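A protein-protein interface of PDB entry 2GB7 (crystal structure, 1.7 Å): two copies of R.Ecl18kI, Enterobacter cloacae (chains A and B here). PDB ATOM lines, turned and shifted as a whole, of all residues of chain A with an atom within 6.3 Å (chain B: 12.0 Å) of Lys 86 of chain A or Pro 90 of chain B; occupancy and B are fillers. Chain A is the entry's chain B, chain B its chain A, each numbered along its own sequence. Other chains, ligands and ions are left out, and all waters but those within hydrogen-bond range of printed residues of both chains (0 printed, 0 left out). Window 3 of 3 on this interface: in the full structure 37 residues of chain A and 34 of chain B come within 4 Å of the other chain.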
ATOM      1  N   ILE A  80     -36.384  23.929 -12.133  1.00  0.00           N
ATOM      2  CA  ILE A  80     -35.172  23.113 -12.100  1.00  0.00           C
ATOM      3  C   ILE A  80     -35.548  21.631 -12.151  1.00  0.00           C
ATOM      4  O   ILE A  80     -36.395  21.164 -11.385  1.00  0.00           O
ATOM      5  CB  ILE A  80     -34.277  23.405 -10.879  1.00  0.00           C
ATOM      6  CG1 ILE A  80     -33.904  24.880 -10.819  1.00  0.00           C
ATOM      7  CG2 ILE A  80     -32.982  22.605 -10.985  1.00  0.00           C
ATOM      8  CD1 ILE A  80     -33.155  25.266  -9.553  1.00  0.00           C
ATOM      9  N   ASP A  81     -34.899  20.899 -13.060  1.00  0.00           N
ATOM     10  CA  ASP A  81     -35.246  19.524 -13.351  1.00  0.00           C
ATOM     11  C   ASP A  81     -34.011  18.676 -13.067  1.00  0.00           C
ATOM     12  O   ASP A  81     -33.063  18.645 -13.859  1.00  0.00           O
ATOM     13  CB  ASP A  81     -35.688  19.410 -14.815  1.00  0.00           C
ATOM     14  CG  ASP A  81     -36.262  18.036 -15.174  1.00  0.00           C
ATOM     15  OD1 ASP A  81     -35.906  17.025 -14.543  1.00  0.00           O
ATOM     16  OD2 ASP A  81     -37.073  17.984 -16.127  1.00  0.00           O
ATOM     17  N   GLU A  82     -34.026  18.023 -11.910  1.00  0.00           N
ATOM     18  CA  GLU A  82     -32.893  17.232 -11.454  1.00  0.00           C
ATOM     19  C   GLU A  82     -32.630  16.052 -12.373  1.00  0.00           C
ATOM     20  O   GLU A  82     -31.473  15.798 -12.725  1.00  0.00           O
ATOM     21  CB  GLU A  82     -33.096  16.793  -9.998  1.00  0.00           C
ATOM     22  CG  GLU A  82     -32.125  15.729  -9.452  1.00  0.00           C
ATOM     23  CD  GLU A  82     -30.647  15.973  -9.774  1.00  0.00           C
ATOM     24  OE1 GLU A  82     -30.241  17.123 -10.036  1.00  0.00           O
ATOM     25  OE2 GLU A  82     -29.884  14.987  -9.761  1.00  0.00           O
ATOM     26  N   GLU A  83     -33.687  15.345 -12.774  1.00  0.00           N
ATOM     27  CA  GLU A  83     -33.523  14.132 -13.594  1.00  0.00           C
ATOM     28  C   GLU A  83     -32.922  14.495 -14.945  1.00  0.00           C
ATOM     29  O   GLU A  83     -32.140  13.736 -15.521  1.00  0.00           O
ATOM     30  CB  GLU A  83     -34.862  13.409 -13.794  1.00  0.00           C
ATOM     31  CG  GLU A  83     -35.313  12.554 -12.615  1.00  0.00           C
ATOM     32  N   ARG A  84     -33.300  15.675 -15.432  1.00  0.00           N
ATOM     33  CA  ARG A  84     -32.799  16.223 -16.676  1.00  0.00           C
ATOM     34  C   ARG A  84     -31.301  16.545 -16.630  1.00  0.00           C
ATOM     35  O   ARG A  84     -30.547  16.168 -17.531  1.00  0.00           O
ATOM     36  CB  ARG A  84     -33.589  17.489 -17.017  1.00  0.00           C
ATOM     37  CG  ARG A  84     -33.590  17.823 -18.475  1.00  0.00           C
ATOM     38  CD  ARG A  84     -34.312  19.128 -18.749  1.00  0.00           C
ATOM     39  NE  ARG A  84     -33.653  19.837 -19.840  1.00  0.00           N
ATOM     40  CZ  ARG A  84     -33.753  19.512 -21.125  1.00  0.00           C
ATOM     41  NH1 ARG A  84     -34.499  18.480 -21.516  1.00  0.00           N
ATOM     42  NH2 ARG A  84     -33.097  20.221 -22.029  1.00  0.00           N
ATOM     43  N   ILE A  85     -30.872  17.203 -15.560  1.00  0.00           N
ATOM     44  CA  ILE A  85     -29.556  17.830 -15.507  1.00  0.00           C
ATOM     45  C   ILE A  85     -28.485  16.980 -14.832  1.00  0.00           C
ATOM     46  O   ILE A  85     -27.321  17.382 -14.755  1.00  0.00           O
ATOM     47  CB  ILE A  85     -29.657  19.191 -14.808  1.00  0.00           C
ATOM     48  CG1 ILE A  85     -30.378  20.170 -15.725  1.00  0.00           C
ATOM     49  CG2 ILE A  85     -28.286  19.727 -14.466  1.00  0.00           C
ATOM     50  CD1 ILE A  85     -31.241  21.176 -14.993  1.00  0.00           C
ATOM     51  N   LYS A  86     -28.888  15.802 -14.361  1.00  0.00           N
ATOM     52  CA  LYS A  86     -28.016  14.869 -13.635  1.00  0.00           C
ATOM     53  C   LYS A  86     -26.543  14.783 -14.061  1.00  0.00           C
ATOM     54  O   LYS A  86     -25.642  14.852 -13.220  1.00  0.00           O
ATOM     55  CB  LYS A  86     -28.624  13.459 -13.644  1.00  0.00           C
ATOM     56  CG  LYS A  86     -29.769  13.296 -12.662  1.00  0.00           C
ATOM     57  CD  LYS A  86     -29.832  11.886 -12.095  1.00  0.00           C
ATOM     58  CE  LYS A  86     -30.418  11.899 -10.682  1.00  0.00           C
ATOM     59  NZ  LYS A  86     -31.778  12.520 -10.596  1.00  0.00           N
ATOM     60  N   ASP A  87     -26.305  14.622 -15.357  1.00  0.00           N
ATOM     61  CA  ASP A  87     -24.980  14.227 -15.857  1.00  0.00           C
ATOM     62  C   ASP A  87     -24.327  15.293 -16.725  1.00  0.00           C
ATOM     63  O   ASP A  87     -23.395  15.014 -17.487  1.00  0.00           O
ATOM     64  CB  ASP A  87     -25.081  12.916 -16.635  1.00  0.00           C
ATOM     65  CG  ASP A  87     -25.639  11.786 -15.801  1.00  0.00           C
ATOM     66  OD1 ASP A  87     -25.302  11.694 -14.595  1.00  0.00           O
ATOM     67  OD2 ASP A  87     -26.425  10.995 -16.362  1.00  0.00           O
ATOM     68  N   MET A  88     -24.819  16.519 -16.606  1.00  0.00           N
ATOM     69  CA  MET A  88     -24.210  17.629 -17.303  1.00  0.00           C
ATOM     70  C   MET A  88     -23.183  18.273 -16.389  1.00  0.00           C
ATOM     71  O   MET A  88     -23.292  18.188 -15.150  1.00  0.00           O
ATOM     72  CB  MET A  88     -25.265  18.679 -17.663  1.00  0.00           C
ATOM     73  CG  MET A  88     -26.518  18.137 -18.349  1.00  0.00           C
ATOM     74  SD  MET A  88     -27.729  19.441 -18.686  1.00  0.00           S
ATOM     75  CE  MET A  88     -27.047  20.145 -20.176  1.00  0.00           C
ATOM     76  N   SER A  89     -22.206  18.946 -16.999  1.00  0.00           N
ATOM     77  CA  SER A  89     -21.306  19.821 -16.260  1.00  0.00           C
ATOM     78  C   SER A  89     -22.155  20.950 -15.685  1.00  0.00           C
ATOM     79  O   SER A  89     -23.233  21.220 -16.200  1.00  0.00           O
ATOM     80  CB  SER A  89     -20.249  20.415 -17.187  1.00  0.00           C
ATOM     81  OG  SER A  89     -20.867  21.237 -18.191  1.00  0.00           O
ATOM     82  N   PRO A  90     -21.688  21.582 -14.599  1.00  0.00           N
ATOM     83  CA  PRO A  90     -22.394  22.779 -14.116  1.00  0.00           C
ATOM     84  C   PRO A  90     -22.592  23.859 -15.189  1.00  0.00           C
ATOM     85  O   PRO A  90     -23.644  24.531 -15.212  1.00  0.00           O
ATOM     86  CB  PRO A  90     -21.484  23.294 -12.989  1.00  0.00           C
ATOM     87  CG  PRO A  90     -20.215  22.520 -13.086  1.00  0.00           C
ATOM     88  CD  PRO A  90     -20.552  21.230 -13.737  1.00  0.00           C
ATOM     89  N   ALA A  93     -25.291  22.709 -17.499  1.00  0.00           N
ATOM     90  CA  ALA A  93     -26.537  22.730 -16.743  1.00  0.00           C
ATOM     91  C   ALA A  93     -27.195  24.118 -16.861  1.00  0.00           C
ATOM     92  O   ALA A  93     -28.366  24.243 -17.251  1.00  0.00           O
ATOM     93  CB  ALA A  93     -26.273  22.396 -15.296  1.00  0.00           C
ATOM     94  N   ILE A  94     -26.425  25.154 -16.534  1.00  0.00           N
ATOM     95  CA  ILE A  94     -26.893  26.532 -16.655  1.00  0.00           C
ATOM     96  C   ILE A  94     -27.248  26.853 -18.102  1.00  0.00           C
ATOM     97  O   ILE A  94     -28.332  27.381 -18.378  1.00  0.00           O
ATOM     98  CB  ILE A  94     -25.853  27.541 -16.117  1.00  0.00           C
ATOM     99  CG1 ILE A  94     -25.688  27.362 -14.607  1.00  0.00           C
ATOM    100  CG2 ILE A  94     -26.269  28.984 -16.464  1.00  0.00           C
ATOM    101  CD1 ILE A  94     -24.323  27.745 -14.084  1.00  0.00           C
ATOM    102  N   ILE B  80     -22.780  33.545 -17.322  1.00  0.00           N
ATOM    103  CA  ILE B  80     -22.288  32.261 -16.824  1.00  0.00           C
ATOM    104  C   ILE B  80     -20.782  32.324 -16.532  1.00  0.00           C
ATOM    105  O   ILE B  80     -19.959  32.615 -17.418  1.00  0.00           O
ATOM    106  CB  ILE B  80     -22.613  31.057 -17.755  1.00  0.00           C
ATOM    107  CG1 ILE B  80     -24.019  31.201 -18.385  1.00  0.00           C
ATOM    108  CG2 ILE B  80     -22.428  29.726 -16.970  1.00  0.00           C
ATOM    109  CD1 ILE B  80     -24.344  30.013 -19.354  1.00  0.00           C
ATOM    110  N   ASP B  81     -20.448  32.012 -15.280  1.00  0.00           N
ATOM    111  CA  ASP B  81     -19.115  32.196 -14.728  1.00  0.00           C
ATOM    112  C   ASP B  81     -18.469  30.834 -14.476  1.00  0.00           C
ATOM    113  O   ASP B  81     -18.698  30.195 -13.437  1.00  0.00           O
ATOM    114  CB  ASP B  81     -19.238  33.022 -13.435  1.00  0.00           C
ATOM    115  CG  ASP B  81     -17.887  33.446 -12.841  1.00  0.00           C
ATOM    116  OD1 ASP B  81     -17.906  34.352 -11.971  1.00  0.00           O
ATOM    117  OD2 ASP B  81     -16.832  32.897 -13.216  1.00  0.00           O
ATOM    118  N   GLU B  82     -17.654  30.400 -15.442  1.00  0.00           N
ATOM    119  CA  GLU B  82     -17.049  29.081 -15.442  1.00  0.00           C
ATOM    120  C   GLU B  82     -16.269  28.838 -14.159  1.00  0.00           C
ATOM    121  O   GLU B  82     -16.410  27.782 -13.545  1.00  0.00           O
ATOM    122  CB  GLU B  82     -16.137  28.890 -16.663  1.00  0.00           C
ATOM    123  CG  GLU B  82     -16.877  28.770 -17.993  1.00  0.00           C
ATOM    124  N   ARG B  84     -16.462  30.317 -11.164  1.00  0.00           N
ATOM    125  CA  ARG B  84     -17.313  30.293  -9.976  1.00  0.00           C
ATOM    126  C   ARG B  84     -18.026  28.949  -9.806  1.00  0.00           C
ATOM    127  O   ARG B  84     -18.177  28.457  -8.684  1.00  0.00           O
ATOM    128  CB  ARG B  84     -18.326  31.438 -10.014  1.00  0.00           C
ATOM    129  CG  ARG B  84     -19.170  31.582  -8.753  1.00  0.00           C
ATOM    130  CD  ARG B  84     -19.864  32.935  -8.705  1.00  0.00           C
ATOM    131  NE  ARG B  84     -20.680  33.090  -7.493  1.00  0.00           N
ATOM    132  N   ILE B  85     -18.416  28.340 -10.921  1.00  0.00           N
ATOM    133  CA  ILE B  85     -19.301  27.177 -10.897  1.00  0.00           C
ATOM    134  C   ILE B  85     -18.581  25.857 -11.081  1.00  0.00           C
ATOM    135  O   ILE B  85     -19.201  24.801 -10.936  1.00  0.00           O
ATOM    136  CB  ILE B  85     -20.428  27.304 -11.956  1.00  0.00           C
ATOM    137  CG1 ILE B  85     -19.838  27.169 -13.377  1.00  0.00           C
ATOM    138  CG2 ILE B  85     -21.177  28.600 -11.736  1.00  0.00           C
ATOM    139  CD1 ILE B  85     -20.854  27.235 -14.503  1.00  0.00           C
ATOM    140  N   LYS B  86     -17.283  25.915 -11.407  1.00  0.00           N
ATOM    141  CA  LYS B  86     -16.478  24.729 -11.681  1.00  0.00           C
ATOM    142  C   LYS B  86     -16.358  23.859 -10.433  1.00  0.00           C
ATOM    143  O   LYS B  86     -15.857  24.301  -9.398  1.00  0.00           O
ATOM    144  CB  LYS B  86     -15.091  25.113 -12.232  1.00  0.00           C
ATOM    145  CG  LYS B  86     -14.165  25.809 -11.230  1.00  0.00           C
ATOM    146  CD  LYS B  86     -12.776  26.063 -11.805  1.00  0.00           C
ATOM    147  CE  LYS B  86     -11.805  26.411 -10.648  1.00  0.00           C
ATOM    148  NZ  LYS B  86     -10.645  27.224 -11.121  1.00  0.00           N
ATOM    149  N   ASP B  87     -16.843  22.627 -10.536  1.00  0.00           N
ATOM    150  CA  ASP B  87     -16.887  21.687  -9.400  1.00  0.00           C
ATOM    151  C   ASP B  87     -18.130  21.856  -8.519  1.00  0.00           C
ATOM    152  O   ASP B  87     -18.234  21.215  -7.469  1.00  0.00           O
ATOM    153  CB  ASP B  87     -15.600  21.723  -8.549  1.00  0.00           C
ATOM    154  CG  ASP B  87     -14.372  21.264  -9.316  1.00  0.00           C
ATOM    155  N   MET B  88     -19.062  22.713  -8.934  1.00  0.00           N
ATOM    156  CA  MET B  88     -20.405  22.692  -8.374  1.00  0.00           C
ATOM    157  C   MET B  88     -21.167  21.505  -8.957  1.00  0.00           C
ATOM    158  O   MET B  88     -20.851  21.031 -10.073  1.00  0.00           O
ATOM    159  CB  MET B  88     -21.171  23.980  -8.696  1.00  0.00           C
ATOM    160  CG  MET B  88     -20.985  25.112  -7.690  1.00  0.00           C
ATOM    161  SD  MET B  88     -22.147  26.409  -8.092  1.00  0.00           S
ATOM    162  CE  MET B  88     -21.696  27.763  -6.978  1.00  0.00           C
ATOM    163  N   SER B  89     -22.146  21.013  -8.189  1.00  0.00           N
ATOM    164  CA  SER B  89     -23.138  20.088  -8.729  1.00  0.00           C
ATOM    165  C   SER B  89     -23.980  20.864  -9.748  1.00  0.00           C
ATOM    166  O   SER B  89     -24.193  22.070  -9.585  1.00  0.00           O
ATOM    167  CB  SER B  89     -23.895  19.386  -7.594  1.00  0.00           C
ATOM    168  OG  SER B  89     -25.000  20.163  -7.150  1.00  0.00           O
ATOM    169  N   PRO B  90     -24.447  20.183 -10.813  1.00  0.00           N
ATOM    170  CA  PRO B  90     -25.243  20.854 -11.852  1.00  0.00           C
ATOM    171  C   PRO B  90     -26.501  21.517 -11.289  1.00  0.00           C
ATOM    172  O   PRO B  90     -26.870  22.620 -11.722  1.00  0.00           O
ATOM    173  CB  PRO B  90     -25.624  19.712 -12.796  1.00  0.00           C
ATOM    174  CG  PRO B  90     -24.665  18.628 -12.522  1.00  0.00           C
ATOM    175  CD  PRO B  90     -24.254  18.753 -11.103  1.00  0.00           C
ATOM    176  N   TYR B  91     -27.142  20.855 -10.325  1.00  0.00           N
ATOM    177  CA  TYR B  91     -28.292  21.435  -9.625  1.00  0.00           C
ATOM    178  C   TYR B  91     -27.895  22.681  -8.835  1.00  0.00           C
ATOM    179  O   TYR B  91     -28.599  23.689  -8.861  1.00  0.00           O
ATOM    180  CB  TYR B  91     -28.925  20.404  -8.679  1.00  0.00           C
ATOM    181  CG  TYR B  91     -29.929  21.027  -7.724  1.00  0.00           C
ATOM    182  CD1 TYR B  91     -31.240  21.269  -8.115  1.00  0.00           C
ATOM    183  CD2 TYR B  91     -29.553  21.371  -6.422  1.00  0.00           C
ATOM    184  CE1 TYR B  91     -32.157  21.852  -7.236  1.00  0.00           C
ATOM    185  CE2 TYR B  91     -30.456  21.959  -5.539  1.00  0.00           C
ATOM    186  CZ  TYR B  91     -31.753  22.180  -5.943  1.00  0.00           C
ATOM    187  OH  TYR B  91     -32.641  22.756  -5.060  1.00  0.00           O
ATOM    188  N   ASP B  92     -26.777  22.590  -8.111  1.00  0.00           N
ATOM    189  CA  ASP B  92     -26.276  23.729  -7.339  1.00  0.00           C
ATOM    190  C   ASP B  92     -25.816  24.883  -8.228  1.00  0.00           C
ATOM    191  O   ASP B  92     -25.993  26.047  -7.877  1.00  0.00           O
ATOM    192  CB  ASP B  92     -25.176  23.301  -6.371  1.00  0.00           C
ATOM    193  CG  ASP B  92     -25.729  22.564  -5.160  1.00  0.00           C
ATOM    194  OD1 ASP B  92     -26.960  22.596  -4.951  1.00  0.00           O
ATOM    195  OD2 ASP B  92     -24.942  21.964  -4.416  1.00  0.00           O
ATOM    196  N   ALA B  93     -25.226  24.551  -9.375  1.00  0.00           N
ATOM    197  CA  ALA B  93     -24.926  25.557 -10.406  1.00  0.00           C
ATOM    198  C   ALA B  93     -26.158  26.351 -10.884  1.00  0.00           C
ATOM    199  O   ALA B  93     -26.112  27.600 -10.963  1.00  0.00           O
ATOM    200  CB  ALA B  93     -24.197  24.901 -11.574  1.00  0.00           C
ATOM    201  N   ILE B  94     -27.275  25.675 -11.157  1.00  0.00           N
ATOM    202  CA  ILE B  94     -28.486  26.395 -11.568  1.00  0.00           C
ATOM    203  C   ILE B  94     -29.076  27.207 -10.415  1.00  0.00           C
ATOM    204  O   ILE B  94     -29.333  28.395 -10.574  1.00  0.00           O
ATOM    205  CB  ILE B  94     -29.556  25.492 -12.221  1.00  0.00           C
ATOM    206  CG1 ILE B  94     -28.990  24.909 -13.522  1.00  0.00           C
ATOM    207  CG2 ILE B  94     -30.861  26.274 -12.444  1.00  0.00           C
ATOM    208  CD1 ILE B  94     -29.862  23.875 -14.197  1.00  0.00           C
ATOM    209  N   ARG B  95     -29.259  26.567  -9.261  1.00  0.00           N
ATOM    210  CA  ARG B  95     -29.668  27.273  -8.040  1.00  0.00           C
ATOM    211  C   ARG B  95     -28.830  28.522  -7.826  1.00  0.00           C
ATOM    212  O   ARG B  95     -29.387  29.592  -7.662  1.00  0.00           O
ATOM    213  CB  ARG B  95     -29.562  26.367  -6.809  1.00  0.00           C
ATOM    214  CG  ARG B  95     -30.675  25.336  -6.689  1.00  0.00           C
ATOM    215  CD  ARG B  95     -31.913  25.884  -6.002  1.00  0.00           C
ATOM    216  NE  ARG B  95     -31.652  26.268  -4.616  1.00  0.00           N
ATOM    217  N   ASP B  96     -27.497  28.384  -7.857  1.00  0.00           N
ATOM    218  CA  ASP B  96     -26.610  29.540  -7.717  1.00  0.00           C
ATOM    219  C   ASP B  96     -26.950  30.611  -8.747  1.00  0.00           C
ATOM    220  O   ASP B  96     -27.133  31.767  -8.401  1.00  0.00           O
ATOM    221  CB  ASP B  96     -25.128  29.172  -7.798  1.00  0.00           C
ATOM    222  CG  ASP B  96     -24.216  30.383  -7.586  1.00  0.00           C
ATOM    223  OD1 ASP B  96     -24.202  30.953  -6.458  1.00  0.00           O
ATOM    224  OD2 ASP B  96     -23.528  30.783  -8.556  1.00  0.00           O
ATOM    225  N   PHE B  97     -27.046  30.210 -10.012  1.00  0.00           N
ATOM    226  CA  PHE B  97     -27.422  31.136 -11.084  1.00  0.00           C
ATOM    227  C   PHE B  97     -28.745  31.864 -10.835  1.00  0.00           C
ATOM    228  O   PHE B  97     -28.858  33.053 -11.124  1.00  0.00           O
ATOM    229  CB  PHE B  97     -27.467  30.398 -12.421  1.00  0.00           C
ATOM    230  CG  PHE B  97     -27.554  31.306 -13.618  1.00  0.00           C
ATOM    231  CD1 PHE B  97     -26.407  31.911 -14.133  1.00  0.00           C
ATOM    232  CD2 PHE B  97     -28.755  31.491 -14.279  1.00  0.00           C
ATOM    233  CE1 PHE B  97     -26.486  32.741 -15.264  1.00  0.00           C
ATOM    234  CE2 PHE B  97     -28.844  32.326 -15.409  1.00  0.00           C
ATOM    235  CZ  PHE B  97     -27.687  32.930 -15.905  1.00  0.00           C
ATOM    236  N   THR B  98     -29.750  31.156 -10.315  1.00  0.00           N
ATOM    237  CA  THR B  98     -31.046  31.760 -10.006  1.00  0.00           C
ATOM    238  C   THR B  98     -31.009  32.637  -8.752  1.00  0.00           C
ATOM    239  O   THR B  98     -31.924  33.394  -8.528  1.00  0.00           O
ATOM    240  CB  THR B  98     -32.208  30.718  -9.850  1.00  0.00           C
ATOM    241  OG1 THR B  98     -32.008  29.899  -8.673  1.00  0.00           O
ATOM    242  CG2 THR B  98     -32.315  29.822 -11.078  1.00  0.00           C
ATOM    243  N   MET B  99     -29.960  32.491  -7.938  1.00  0.00           N
ATOM    244  CA  MET B  99     -29.776  33.283  -6.717  1.00  0.00           C
ATOM    245  C   MET B  99     -28.874  34.487  -6.964  1.00  0.00           C
ATOM    246  O   MET B  99     -29.113  35.573  -6.428  1.00  0.00           O
ATOM    247  CB  MET B  99     -29.166  32.431  -5.600  1.00  0.00           C
ATOM    248  CG  MET B  99     -30.004  31.256  -5.139  1.00  0.00           C
ATOM    249  SD  MET B  99     -29.490  30.645  -3.523  1.00  0.00           S
ATOM    250  CE  MET B  99     -30.518  31.704  -2.499  1.00  0.00           C
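Tyr 91 of chain B touches Ile 80 of chain A (CD1 to CG2, 3.6 Å). Ile 94 of chain B touches Ile 80 of chain A (CG2 to CG1, 3.7 Å). CD1 of Ile 85 of chain A touches CD1 of Ile 94 of chain B (3.1 Å). Met 88 of chain A touches Pro 90 of chain B. Pro 90 of chain A touches Ile 85 of chain B. CB of Ala 93 of chain A touches O of Pro 90 of chain B, at 3.6 Å. CD1 of Ile 80 of chain B touches CG2 of Ile 94 of chain A (3.6 Å). Ile 85 of chain B touches Ile 94 of chain A. CG1 of Ile 94 of chain B touches N of Ile 94 of chain A, at 3.96 Å. CG2 of Ile 94 of chain A touches CD1 of Phe 97 of chain B (3.7 Å).
The side-chain hydroxyl of Thr 98 of chain B sits at hydrogen-bond distance from the backbone carbonyl oxygen of Arg 95 of chain B (2.8 Å). OE2 of Glu 82 of chain A lies within salt-bridge range of NZ of Lys 86 of chain A (3.2 Å).
Ile 80 of chain A touches Ile 94 of chain B, and with the chains exchanged Ile 94 of chain A touches Ile 80 of chain B. Lys 86 of chain A touches Pro 90 of chain B, but with the chains exchanged Pro 90 of chain A does not touch Lys 86 of chain B (4.6 Å). Ala 93 of chain A touches Ile 94 of chain B, and with the chains exchanged Ile 94 of chain A touches Ala 93 of chain B. Ile 94 of chain A touches its own counterpart, Ile 94 of chain B. Of the 18 pairs that touch across the chains among the printed residues, 13 have their exchanged pair printed and touching as well.
Of the 19 printed residues of chain B, 9 touch a printed residue of chain A. Hydrophobic or aromatic side chains of chain B that line the printed part of chain A: Ile 80, Ile 85, Pro 90, Tyr 91, Ala 93, Ile 94 and Phe 97. Of the 13 printed residues of chain A, 8 touch a printed residue of chain B. Among the printed residues, no Asp or Glu carboxylate lies within 4 Å of a Lys or Arg side-chain nitrogen of the other chain.
Lys 86 of chain A touches just one residue of chain B: Pro 90 (3.96 Å). Printed residues of chain A within 4 Å of Pro 90 of chain B: Ile 85, Lys 86, Met 88 and Ala 93. Of chain B, only Tyr 91 (3.8 Å) comes within 4 Å of Glu 82 of chain A. No residue of chain B comes within 4 Å of Glu 83 of chain A. Asp 87 of chain A touches none of the printed residues of chain B. Of chain B, only Pro 90 and Ile 94 come within 4 Å of Ala 93 of chain A. Printed residues of chain A within 4 Å of Ile 80 of chain B: Ile 94 (3.6 Å). Of the printed residues of chain A, Ala 93 of chain B touches Pro 90 and Ile 94. Of the printed residues of chain A, Phe 97 of chain B touches Ile 94. Of the printed residues of chain A, Arg 95 of chain B touches Ile 80 (3.8 Å). The nearest residue of chain A that does not touch Pro 90 of chain B is Pro 90 of chain A (4.1 Å). The nearest printed residue of chain A that does not touch Tyr 91 of chain B is Ile 85 of chain A (4.4 Å).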
